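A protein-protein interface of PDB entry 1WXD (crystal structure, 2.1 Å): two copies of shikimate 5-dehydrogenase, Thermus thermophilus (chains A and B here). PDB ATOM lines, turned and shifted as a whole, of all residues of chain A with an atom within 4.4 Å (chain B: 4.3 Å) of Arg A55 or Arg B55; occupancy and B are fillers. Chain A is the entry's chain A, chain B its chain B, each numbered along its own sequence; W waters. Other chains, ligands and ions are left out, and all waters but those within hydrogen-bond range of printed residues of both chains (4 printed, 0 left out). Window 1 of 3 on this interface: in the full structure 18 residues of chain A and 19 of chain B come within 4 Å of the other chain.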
ATOM      1  N   LEU A   2      -4.362 -12.045 -25.276  1.00  0.00           N
ATOM      2  CA  LEU A   2      -5.041 -13.318 -25.116  1.00  0.00           C
ATOM      3  C   LEU A   2      -4.254 -14.455 -24.499  1.00  0.00           C
ATOM      4  O   LEU A   2      -3.835 -15.382 -25.193  1.00  0.00           O
ATOM      5  CB  LEU A   2      -5.587 -13.777 -26.461  1.00  0.00           C
ATOM      6  CG  LEU A   2      -6.505 -12.760 -27.138  1.00  0.00           C
ATOM      7  CD1 LEU A   2      -7.168 -13.418 -28.332  1.00  0.00           C
ATOM      8  CD2 LEU A   2      -7.555 -12.258 -26.152  1.00  0.00           C
ATOM      9  N   ARG A   3      -4.050 -14.382 -23.191  1.00  0.00           N
ATOM     10  CA  ARG A   3      -3.418 -15.457 -22.510  1.00  0.00           C
ATOM     11  C   ARG A   3      -4.372 -15.855 -21.436  1.00  0.00           C
ATOM     12  O   ARG A   3      -4.793 -15.052 -20.614  1.00  0.00           O
ATOM     13  CB  ARG A   3      -2.118 -14.942 -21.890  1.00  0.00           C
ATOM     14  CG  ARG A   3      -1.126 -16.069 -21.599  1.00  0.00           C
ATOM     15  CD  ARG A   3      -0.319 -15.814 -20.319  1.00  0.00           C
ATOM     16  NE  ARG A   3       0.744 -14.834 -20.564  1.00  0.00           N
ATOM     17  CZ  ARG A   3       1.192 -14.131 -19.507  1.00  0.00           C
ATOM     18  NH1 ARG A   3       0.687 -14.344 -18.304  1.00  0.00           N
ATOM     19  NH2 ARG A   3       2.129 -13.195 -19.685  1.00  0.00           N
ATOM     20  N   PHE A   4      -4.789 -17.110 -21.480  1.00  0.00           N
ATOM     21  CA  PHE A   4      -5.756 -17.596 -20.520  1.00  0.00           C
ATOM     22  C   PHE A   4      -5.159 -18.769 -19.761  1.00  0.00           C
ATOM     23  O   PHE A   4      -4.020 -19.168 -20.004  1.00  0.00           O
ATOM     24  CB  PHE A   4      -7.032 -18.038 -21.234  1.00  0.00           C
ATOM     25  CG  PHE A   4      -7.558 -17.036 -22.225  1.00  0.00           C
ATOM     26  CD1 PHE A   4      -7.196 -17.108 -23.565  1.00  0.00           C
ATOM     27  CD2 PHE A   4      -8.439 -16.038 -21.825  1.00  0.00           C
ATOM     28  CE1 PHE A   4      -7.711 -16.205 -24.495  1.00  0.00           C
ATOM     29  CE2 PHE A   4      -8.958 -15.129 -22.746  1.00  0.00           C
ATOM     30  CZ  PHE A   4      -8.592 -15.216 -24.085  1.00  0.00           C
ATOM     31  N   ALA A  53      -1.326 -10.029 -16.347  1.00  0.00           N
ATOM     32  CA  ALA A  53      -0.956 -10.662 -17.598  1.00  0.00           C
ATOM     33  C   ALA A  53      -1.972 -11.577 -18.263  1.00  0.00           C
ATOM     34  O   ALA A  53      -1.720 -12.067 -19.361  1.00  0.00           O
ATOM     35  CB  ALA A  53       0.341 -11.410 -17.393  1.00  0.00           C
ATOM     36  N   PHE A  54      -3.111 -11.814 -17.622  1.00  0.00           N
ATOM     37  CA  PHE A  54      -4.108 -12.693 -18.218  1.00  0.00           C
ATOM     38  C   PHE A  54      -5.414 -11.994 -18.571  1.00  0.00           C
ATOM     39  O   PHE A  54      -5.970 -11.239 -17.778  1.00  0.00           O
ATOM     40  CB  PHE A  54      -4.399 -13.884 -17.294  1.00  0.00           C
ATOM     41  CG  PHE A  54      -3.252 -14.845 -17.165  1.00  0.00           C
ATOM     42  CD1 PHE A  54      -2.166 -14.550 -16.346  1.00  0.00           C
ATOM     43  CD2 PHE A  54      -3.247 -16.042 -17.882  1.00  0.00           C
ATOM     44  CE1 PHE A  54      -1.088 -15.431 -16.239  1.00  0.00           C
ATOM     45  CE2 PHE A  54      -2.176 -16.932 -17.787  1.00  0.00           C
ATOM     46  CZ  PHE A  54      -1.092 -16.625 -16.962  1.00  0.00           C
ATOM     47  N   ARG A  55      -5.892 -12.255 -19.780  1.00  0.00           N
ATOM     48  CA  ARG A  55      -7.136 -11.673 -20.246  1.00  0.00           C
ATOM     49  C   ARG A  55      -8.284 -12.303 -19.471  1.00  0.00           C
ATOM     50  O   ARG A  55      -9.276 -11.646 -19.173  1.00  0.00           O
ATOM     51  CB  ARG A  55      -7.312 -11.934 -21.743  1.00  0.00           C
ATOM     52  CG  ARG A  55      -8.693 -11.585 -22.284  1.00  0.00           C
ATOM     53  CD  ARG A  55      -9.070 -10.135 -22.016  1.00  0.00           C
ATOM     54  NE  ARG A  55     -10.306  -9.782 -22.713  1.00  0.00           N
ATOM     55  CZ  ARG A  55     -10.774  -8.545 -22.844  1.00  0.00           C
ATOM     56  NH1 ARG A  55     -10.120  -7.518 -22.321  1.00  0.00           N
ATOM     57  NH2 ARG A  55     -11.895  -8.334 -23.516  1.00  0.00           N
ATOM     58  N   GLY A  56      -8.137 -13.582 -19.148  1.00  0.00           N
ATOM     59  CA  GLY A  56      -9.177 -14.273 -18.414  1.00  0.00           C
ATOM     60  C   GLY A  56      -8.766 -15.664 -17.978  1.00  0.00           C
ATOM     61  O   GLY A  56      -7.837 -16.250 -18.542  1.00  0.00           O
ATOM     62  N   LEU A  88     -12.831 -12.462 -15.799  1.00  0.00           N
ATOM     63  CA  LEU A  88     -12.392 -11.599 -16.893  1.00  0.00           C
ATOM     64  C   LEU A  88     -11.534 -10.473 -16.328  1.00  0.00           C
ATOM     65  O   LEU A  88     -11.914  -9.840 -15.341  1.00  0.00           O
ATOM     66  CB  LEU A  88     -13.595 -10.984 -17.612  1.00  0.00           C
ATOM     67  CG  LEU A  88     -13.294  -9.774 -18.507  1.00  0.00           C
ATOM     68  CD1 LEU A  88     -12.573 -10.225 -19.778  1.00  0.00           C
ATOM     69  CD2 LEU A  88     -14.592  -9.075 -18.863  1.00  0.00           C
ATOM     70  N   GLN A  89     -10.383 -10.229 -16.947  1.00  0.00           N
ATOM     71  CA  GLN A  89      -9.503  -9.157 -16.507  1.00  0.00           C
ATOM     72  C   GLN A  89      -9.506  -8.030 -17.528  1.00  0.00           C
ATOM     73  O   GLN A  89      -9.256  -8.246 -18.716  1.00  0.00           O
ATOM     74  CB  GLN A  89      -8.070  -9.669 -16.305  1.00  0.00           C
ATOM     75  CG  GLN A  89      -7.065  -8.600 -15.858  1.00  0.00           C
ATOM     76  CD  GLN A  89      -6.548  -7.739 -17.005  1.00  0.00           C
ATOM     77  OE1 GLN A  89      -6.875  -6.553 -17.107  1.00  0.00           O
ATOM     78  NE2 GLN A  89      -5.734  -8.332 -17.873  1.00  0.00           N
ATOM     79  N   VAL A  90      -9.816  -6.831 -17.053  1.00  0.00           N
ATOM     80  CA  VAL A  90      -9.843  -5.628 -17.876  1.00  0.00           C
ATOM     81  C   VAL A  90      -9.270  -4.496 -17.025  1.00  0.00           C
ATOM     82  O   VAL A  90      -9.694  -4.286 -15.890  1.00  0.00           O
ATOM     83  CB  VAL A  90     -11.285  -5.266 -18.311  1.00  0.00           C
ATOM     84  CG1 VAL A  90     -11.324  -3.835 -18.804  1.00  0.00           C
ATOM     85  CG2 VAL A  90     -11.743  -6.205 -19.416  1.00  0.00           C
ATOM     86  N   ARG A 241     -16.469 -16.337 -25.126  1.00  0.00           N
ATOM     87  CA  ARG A 241     -17.224 -15.194 -25.638  1.00  0.00           C
ATOM     88  C   ARG A 241     -17.140 -14.073 -24.603  1.00  0.00           C
ATOM     89  O   ARG A 241     -17.014 -12.900 -24.940  1.00  0.00           O
ATOM     90  CB  ARG A 241     -18.690 -15.569 -25.877  1.00  0.00           C
ATOM     91  CG  ARG A 241     -19.463 -14.495 -26.634  1.00  0.00           C
ATOM     92  CD  ARG A 241     -20.857 -14.293 -26.058  1.00  0.00           C
ATOM     93  NE  ARG A 241     -21.845 -15.185 -26.657  1.00  0.00           N
ATOM     94  CZ  ARG A 241     -22.867 -15.740 -26.005  1.00  0.00           C
ATOM     95  NH1 ARG A 241     -23.050 -15.514 -24.706  1.00  0.00           N
ATOM     96  NH2 ARG A 241     -23.725 -16.507 -26.664  1.00  0.00           N
ATOM     97  N   LEU A 242     -17.216 -14.449 -23.335  1.00  0.00           N
ATOM     98  CA  LEU A 242     -17.120 -13.493 -22.250  1.00  0.00           C
ATOM     99  C   LEU A 242     -15.830 -12.707 -22.404  1.00  0.00           C
ATOM    100  O   LEU A 242     -15.826 -11.472 -22.373  1.00  0.00           O
ATOM    101  CB  LEU A 242     -17.112 -14.231 -20.920  1.00  0.00           C
ATOM    102  CG  LEU A 242     -18.235 -13.970 -19.932  1.00  0.00           C
ATOM    103  CD1 LEU A 242     -19.568 -13.743 -20.643  1.00  0.00           C
ATOM    104  CD2 LEU A 242     -18.302 -15.160 -18.999  1.00  0.00           C
ATOM    105  N   TRP A 243     -14.738 -13.442 -22.579  1.00  0.00           N
ATOM    106  CA  TRP A 243     -13.412 -12.860 -22.723  1.00  0.00           C
ATOM    107  C   TRP A 243     -13.144 -12.055 -23.995  1.00  0.00           C
ATOM    108  O   TRP A 243     -12.454 -11.033 -23.956  1.00  0.00           O
ATOM    109  CB  TRP A 243     -12.348 -13.965 -22.633  1.00  0.00           C
ATOM    110  CG  TRP A 243     -12.315 -14.701 -21.335  1.00  0.00           C
ATOM    111  CD1 TRP A 243     -12.537 -14.183 -20.089  1.00  0.00           C
ATOM    112  CD2 TRP A 243     -12.008 -16.086 -21.146  1.00  0.00           C
ATOM    113  NE1 TRP A 243     -12.390 -15.162 -19.139  1.00  0.00           N
ATOM    114  CE2 TRP A 243     -12.065 -16.340 -19.758  1.00  0.00           C
ATOM    115  CE3 TRP A 243     -11.693 -17.138 -22.014  1.00  0.00           C
ATOM    116  CZ2 TRP A 243     -11.815 -17.608 -19.216  1.00  0.00           C
ATOM    117  CZ3 TRP A 243     -11.445 -18.398 -21.477  1.00  0.00           C
ATOM    118  CH2 TRP A 243     -11.509 -18.621 -20.089  1.00  0.00           C
ATOM    119  N   THR A 244     -13.680 -12.510 -25.119  1.00  0.00           N
ATOM    120  CA  THR A 244     -13.401 -11.841 -26.379  1.00  0.00           C
ATOM    121  C   THR A 244     -14.575 -11.265 -27.147  1.00  0.00           C
ATOM    122  O   THR A 244     -14.395 -10.335 -27.935  1.00  0.00           O
ATOM    123  CB  THR A 244     -12.679 -12.796 -27.326  1.00  0.00           C
ATOM    124  OG1 THR A 244     -13.589 -13.825 -27.739  1.00  0.00           O
ATOM    125  CG2 THR A 244     -11.484 -13.435 -26.626  1.00  0.00           C
ATOM    126  N   GLY A 245     -15.761 -11.831 -26.942  1.00  0.00           N
ATOM    127  CA  GLY A 245     -16.932 -11.365 -27.657  1.00  0.00           C
ATOM    128  C   GLY A 245     -17.203 -12.292 -28.830  1.00  0.00           C
ATOM    129  O   GLY A 245     -18.117 -12.068 -29.626  1.00  0.00           O
ATOM    130  N   ARG B   3     -20.051  -6.122 -32.676  1.00  0.00           N
ATOM    131  CA  ARG B   3     -20.799  -4.908 -32.986  1.00  0.00           C
ATOM    132  C   ARG B   3     -20.420  -3.764 -32.056  1.00  0.00           C
ATOM    133  O   ARG B   3     -20.662  -3.829 -30.850  1.00  0.00           O
ATOM    134  CB  ARG B   3     -22.316  -5.160 -32.889  1.00  0.00           C
ATOM    135  CG  ARG B   3     -22.873  -6.208 -33.847  1.00  0.00           C
ATOM    136  CD  ARG B   3     -22.311  -5.979 -35.231  1.00  0.00           C
ATOM    137  NE  ARG B   3     -23.272  -6.165 -36.287  1.00  0.00           N
ATOM    138  CZ  ARG B   3     -22.995  -6.095 -37.589  1.00  0.00           C
ATOM    139  NH1 ARG B   3     -21.761  -5.845 -37.999  1.00  0.00           N
ATOM    140  NH2 ARG B   3     -23.966  -6.261 -38.503  1.00  0.00           N
ATOM    141  N   PHE B   4     -19.831  -2.715 -32.629  1.00  0.00           N
ATOM    142  CA  PHE B   4     -19.417  -1.550 -31.862  1.00  0.00           C
ATOM    143  C   PHE B   4     -20.036  -0.274 -32.429  1.00  0.00           C
ATOM    144  O   PHE B   4     -20.587  -0.265 -33.532  1.00  0.00           O
ATOM    145  CB  PHE B   4     -17.891  -1.395 -31.892  1.00  0.00           C
ATOM    146  CG  PHE B   4     -17.140  -2.603 -31.421  1.00  0.00           C
ATOM    147  CD1 PHE B   4     -16.429  -3.387 -32.325  1.00  0.00           C
ATOM    148  CD2 PHE B   4     -17.117  -2.943 -30.074  1.00  0.00           C
ATOM    149  CE1 PHE B   4     -15.699  -4.494 -31.891  1.00  0.00           C
ATOM    150  CE2 PHE B   4     -16.394  -4.046 -29.629  1.00  0.00           C
ATOM    151  CZ  PHE B   4     -15.682  -4.824 -30.537  1.00  0.00           C
ATOM    152  N   PHE B  54     -24.717  -5.001 -28.740  1.00  0.00           N
ATOM    153  CA  PHE B  54     -23.352  -4.531 -28.954  1.00  0.00           C
ATOM    154  C   PHE B  54     -22.371  -5.052 -27.912  1.00  0.00           C
ATOM    155  O   PHE B  54     -22.673  -5.101 -26.720  1.00  0.00           O
ATOM    156  CB  PHE B  54     -23.305  -2.996 -28.964  1.00  0.00           C
ATOM    157  CG  PHE B  54     -24.006  -2.373 -30.139  1.00  0.00           C
ATOM    158  CD1 PHE B  54     -25.392  -2.410 -30.238  1.00  0.00           C
ATOM    159  CD2 PHE B  54     -23.279  -1.758 -31.155  1.00  0.00           C
ATOM    160  CE1 PHE B  54     -26.045  -1.848 -31.332  1.00  0.00           C
ATOM    161  CE2 PHE B  54     -23.924  -1.193 -32.255  1.00  0.00           C
ATOM    162  CZ  PHE B  54     -25.310  -1.237 -32.342  1.00  0.00           C
ATOM    163  N   ARG B  55     -21.188  -5.436 -28.376  1.00  0.00           N
ATOM    164  CA  ARG B  55     -20.150  -5.935 -27.490  1.00  0.00           C
ATOM    165  C   ARG B  55     -19.615  -4.757 -26.691  1.00  0.00           C
ATOM    166  O   ARG B  55     -19.195  -4.906 -25.547  1.00  0.00           O
ATOM    167  CB  ARG B  55     -19.015  -6.565 -28.304  1.00  0.00           C
ATOM    168  CG  ARG B  55     -17.758  -6.879 -27.499  1.00  0.00           C
ATOM    169  CD  ARG B  55     -18.009  -7.942 -26.432  1.00  0.00           C
ATOM    170  NE  ARG B  55     -16.786  -8.274 -25.700  1.00  0.00           N
ATOM    171  CZ  ARG B  55     -16.689  -9.241 -24.793  1.00  0.00           C
ATOM    172  NH1 ARG B  55     -17.747  -9.986 -24.492  1.00  0.00           N
ATOM    173  NH2 ARG B  55     -15.529  -9.463 -24.185  1.00  0.00           N
ATOM    174  N   GLY B  56     -19.637  -3.583 -27.312  1.00  0.00           N
ATOM    175  CA  GLY B  56     -19.131  -2.392 -26.641  1.00  0.00           C
ATOM    176  C   GLY B  56     -19.372  -1.116 -27.456  1.00  0.00           C
ATOM    177  O   GLY B  56     -19.693  -1.137 -28.634  1.00  0.00           O
ATOM    178  N   LEU B  88     -18.360  -1.542 -21.872  1.00  0.00           N
ATOM    179  CA  LEU B  88     -18.205  -2.952 -22.222  1.00  0.00           C
ATOM    180  C   LEU B  88     -19.484  -3.701 -21.871  1.00  0.00           C
ATOM    181  O   LEU B  88     -20.048  -3.496 -20.795  1.00  0.00           O
ATOM    182  CB  LEU B  88     -17.038  -3.565 -21.446  1.00  0.00           C
ATOM    183  CG  LEU B  88     -16.957  -5.095 -21.408  1.00  0.00           C
ATOM    184  CD1 LEU B  88     -16.694  -5.646 -22.798  1.00  0.00           C
ATOM    185  CD2 LEU B  88     -15.852  -5.505 -20.458  1.00  0.00           C
ATOM    186  N   GLN B  89     -19.929  -4.576 -22.769  1.00  0.00           N
ATOM    187  CA  GLN B  89     -21.148  -5.351 -22.534  1.00  0.00           C
ATOM    188  C   GLN B  89     -20.895  -6.844 -22.436  1.00  0.00           C
ATOM    189  O   GLN B  89     -20.519  -7.491 -23.412  1.00  0.00           O
ATOM    190  CB  GLN B  89     -22.179  -5.099 -23.640  1.00  0.00           C
ATOM    191  CG  GLN B  89     -23.530  -5.791 -23.403  1.00  0.00           C
ATOM    192  CD  GLN B  89     -23.555  -7.238 -23.860  1.00  0.00           C
ATOM    193  OE1 GLN B  89     -23.644  -8.157 -23.044  1.00  0.00           O
ATOM    194  NE2 GLN B  89     -23.477  -7.449 -25.168  1.00  0.00           N
ATOM    195  N   VAL B  90     -21.108  -7.386 -21.245  1.00  0.00           N
ATOM    196  CA  VAL B  90     -20.930  -8.808 -21.015  1.00  0.00           C
ATOM    197  C   VAL B  90     -22.153  -9.353 -20.301  1.00  0.00           C
ATOM    198  O   VAL B  90     -22.596  -8.789 -19.301  1.00  0.00           O
ATOM    199  CB  VAL B  90     -19.685  -9.091 -20.155  1.00  0.00           C
ATOM    200  CG1 VAL B  90     -19.657 -10.552 -19.755  1.00  0.00           C
ATOM    201  CG2 VAL B  90     -18.427  -8.742 -20.934  1.00  0.00           C
ATOM    202  N   ARG B 241      -9.010  -3.090 -26.997  1.00  0.00           N
ATOM    203  CA  ARG B 241      -8.404  -4.126 -26.162  1.00  0.00           C
ATOM    204  C   ARG B 241      -9.384  -4.511 -25.057  1.00  0.00           C
ATOM    205  O   ARG B 241      -9.580  -5.693 -24.762  1.00  0.00           O
ATOM    206  CB  ARG B 241      -7.096  -3.614 -25.546  1.00  0.00           C
ATOM    207  CG  ARG B 241      -6.338  -4.646 -24.715  1.00  0.00           C
ATOM    208  CD  ARG B 241      -4.958  -4.128 -24.349  1.00  0.00           C
ATOM    209  NE  ARG B 241      -4.142  -5.122 -23.656  1.00  0.00           N
ATOM    210  CZ  ARG B 241      -4.360  -5.547 -22.416  1.00  0.00           C
ATOM    211  NH1 ARG B 241      -5.379  -5.068 -21.715  1.00  0.00           N
ATOM    212  NH2 ARG B 241      -3.554  -6.451 -21.874  1.00  0.00           N
ATOM    213  N   LEU B 242      -9.996  -3.498 -24.455  1.00  0.00           N
ATOM    214  CA  LEU B 242     -10.977  -3.707 -23.399  1.00  0.00           C
ATOM    215  C   LEU B 242     -12.087  -4.623 -23.915  1.00  0.00           C
ATOM    216  O   LEU B 242     -12.473  -5.588 -23.257  1.00  0.00           O
ATOM    217  CB  LEU B 242     -11.583  -2.364 -22.977  1.00  0.00           C
ATOM    218  CG  LEU B 242     -11.397  -1.890 -21.534  1.00  0.00           C
ATOM    219  CD1 LEU B 242      -9.919  -1.887 -21.180  1.00  0.00           C
ATOM    220  CD2 LEU B 242     -11.982  -0.499 -21.369  1.00  0.00           C
ATOM    221  N   TRP B 243     -12.584  -4.320 -25.111  1.00  0.00           N
ATOM    222  CA  TRP B 243     -13.663  -5.090 -25.718  1.00  0.00           C
ATOM    223  C   TRP B 243     -13.333  -6.518 -26.142  1.00  0.00           C
ATOM    224  O   TRP B 243     -14.129  -7.424 -25.915  1.00  0.00           O
ATOM    225  CB  TRP B 243     -14.221  -4.347 -26.936  1.00  0.00           C
ATOM    226  CG  TRP B 243     -14.824  -3.025 -26.613  1.00  0.00           C
ATOM    227  CD1 TRP B 243     -15.536  -2.702 -25.497  1.00  0.00           C
ATOM    228  CD2 TRP B 243     -14.789  -1.846 -27.422  1.00  0.00           C
ATOM    229  NE1 TRP B 243     -15.945  -1.394 -25.556  1.00  0.00           N
ATOM    230  CE2 TRP B 243     -15.503  -0.844 -26.728  1.00  0.00           C
ATOM    231  CE3 TRP B 243     -14.223  -1.537 -28.666  1.00  0.00           C
ATOM    232  CZ2 TRP B 243     -15.667   0.449 -27.238  1.00  0.00           C
ATOM    233  CZ3 TRP B 243     -14.385  -0.253 -29.171  1.00  0.00           C
ATOM    234  CH2 TRP B 243     -15.102   0.725 -28.457  1.00  0.00           C
ATOM    235  N   THR B 244     -12.169  -6.722 -26.755  1.00  0.00           N
ATOM    236  CA  THR B 244     -11.805  -8.049 -27.249  1.00  0.00           C
ATOM    237  C   THR B 244     -10.532  -8.667 -26.675  1.00  0.00           C
ATOM    238  O   THR B 244     -10.290  -9.860 -26.849  1.00  0.00           O
ATOM    239  CB  THR B 244     -11.644  -8.035 -28.785  1.00  0.00           C
ATOM    240  OG1 THR B 244     -10.470  -7.289 -29.134  1.00  0.00           O
ATOM    241  CG2 THR B 244     -12.857  -7.393 -29.446  1.00  0.00           C
ATOM    242  N   GLY B 245      -9.713  -7.864 -26.007  1.00  0.00           N
ATOM    243  CA  GLY B 245      -8.479  -8.394 -25.460  1.00  0.00           C
ATOM    244  C   GLY B 245      -7.328  -8.298 -26.448  1.00  0.00           C
ATOM    245  O   GLY B 245      -6.219  -8.735 -26.155  1.00  0.00           O
HETATM  246  O   HOH W   1      -7.728  -7.201 -20.623  1.00  0.00           O
HETATM  247  O   HOH W   2      -5.682  -9.992 -23.965  1.00  0.00           O
HETATM  248  O   HOH W   3      -4.911  -5.014 -18.820  1.00  0.00           O
HETATM  249  O   HOH W   4      -2.794  -8.064 -19.696  1.00  0.00           O
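NH1 of Arg A55 lies within hydrogen-bond range of O of Arg B241.
NH2 of Arg A55 sits at hydrogen-bond distance from O of Leu B242 (2.8 Å).
O of Trp B243 sits at hydrogen-bond distance from NH2 of Arg A55 (3.4 Å).
NH1 of Arg B55 lies within hydrogen-bond range of O of Arg A241 (3.0 Å).
The guanidinium group (NH2) of Arg B55 is in hydrogen-bond range of the backbone carbonyl oxygen (O) of Leu A242, 2.7 Å away.
The guanidinium group (NH2) of Arg B55 is in hydrogen-bond range of the backbone carbonyl oxygen (O) of Trp A243, at 3.5 Å.
The guanidinium group (NH2) of Arg A55 lies close to the backbone NH (N) of Gly B245, 3.3 Å away.
Among the printed residues, pairs that only touch across the chains: Leu A2 with Thr B244, Leu A2 with Gly B245, Arg A55 with Arg B55, Arg A55 with Thr B244, Val A90 with Leu B242, Leu A242 with Val B90, Trp A243 with Thr B244, Thr A244 with Arg B55, Thr A244 with Trp B243, Thr A244 with Thr B244 and Gly A245 with Arg B55.
Arg A55 touches Thr B244, and with the chains exchanged Thr A244 touches Arg B55.
Arg A55 touches Gly B245, and with the chains exchanged Gly A245 touches Arg B55.
Val A90 touches Leu B242, and with the chains exchanged Leu A242 touches Val B90.
Trp A243 touches Thr B244, and with the chains exchanged Thr A244 touches Trp B243.
Positions printed for both chains: 3, 4, 54, 55, 56, 88, 89, 90, 241, 242, 243, 244 and 245.
Arg A55 touches just these residues of chain B: Arg B55 (3.9 Å), Arg B241 (3.1 Å), Leu B242 (2.8 Å), Trp B243 (3.4 Å), Thr B244 (3.5 Å) and Gly B245 (3.3 Å).
Arg B55 touches six residues of chain A.
Printed residues of chain B within 4 Å of Gly A245: Arg B55.
Printed residues of chain A within 4 Å of Thr B244: Leu A2 (3.7 Å), Arg A55 (3.5 Å), Trp A243 (3.8 Å) and Thr A244 (3.5 Å).
Printed residues of chain B within 4 Å of Val A90: Leu B242.
The nearest printed residue of chain B that does not touch Arg A55 is Leu B88 (5.5 Å).
The nearest printed residue of chain A that does not touch Arg B55 is Leu A88 (5.4 Å).
The nearest printed residue of chain B that does not touch Leu A2 is Arg B241 (6.6 Å).
Hydrophobic or aromatic side chains of chain B within 4 Å of the printed part of chain A: Val B90 and Leu B242.
Hydrophobic or aromatic side chains of chain A within 4 Å of the printed part of chain B: Leu A2, Val A90 and Leu A242.
O of Arg A3 is in hydrogen-bond range of N of Arg A55 (3.1 Å).
O of Arg A55 lies within hydrogen-bond range of N of Gln A89 (2.9 Å).
The guanidinium group (NE) of Arg A55 is in hydrogen-bond range of the backbone carbonyl oxygen (O) of Trp A243 (2.8 Å).
The backbone carbonyl oxygen (O) of Arg B3 lies within hydrogen-bond range of the backbone NH (N) of Arg B55, 3.0 Å away.
O of Arg B55 sits at hydrogen-bond distance from N of Gln B89.
The guanidinium group of Arg B55 sits at hydrogen-bond distance from the backbone carbonyl oxygen of Trp B243.
Water W2 bridges O of Gly B245 (2.6 Å) and N of Leu A2 (2.8 Å).
Water W1 lies within hydrogen-bond range of the backbone carbonyl oxygen of Gln A89, the guanidinium group of Arg A55 and the guanidinium group of Arg B241.
Water W4 bridges the guanidinium group of Arg B241 (2.8 Å) and the side-chain amide nitrogen of Gln A89 (3.5 Å).
Water W3 lies within hydrogen-bond range of NH1 of Arg B241 (2.9 Å) and OE1 of Gln A89 (3.0 Å).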
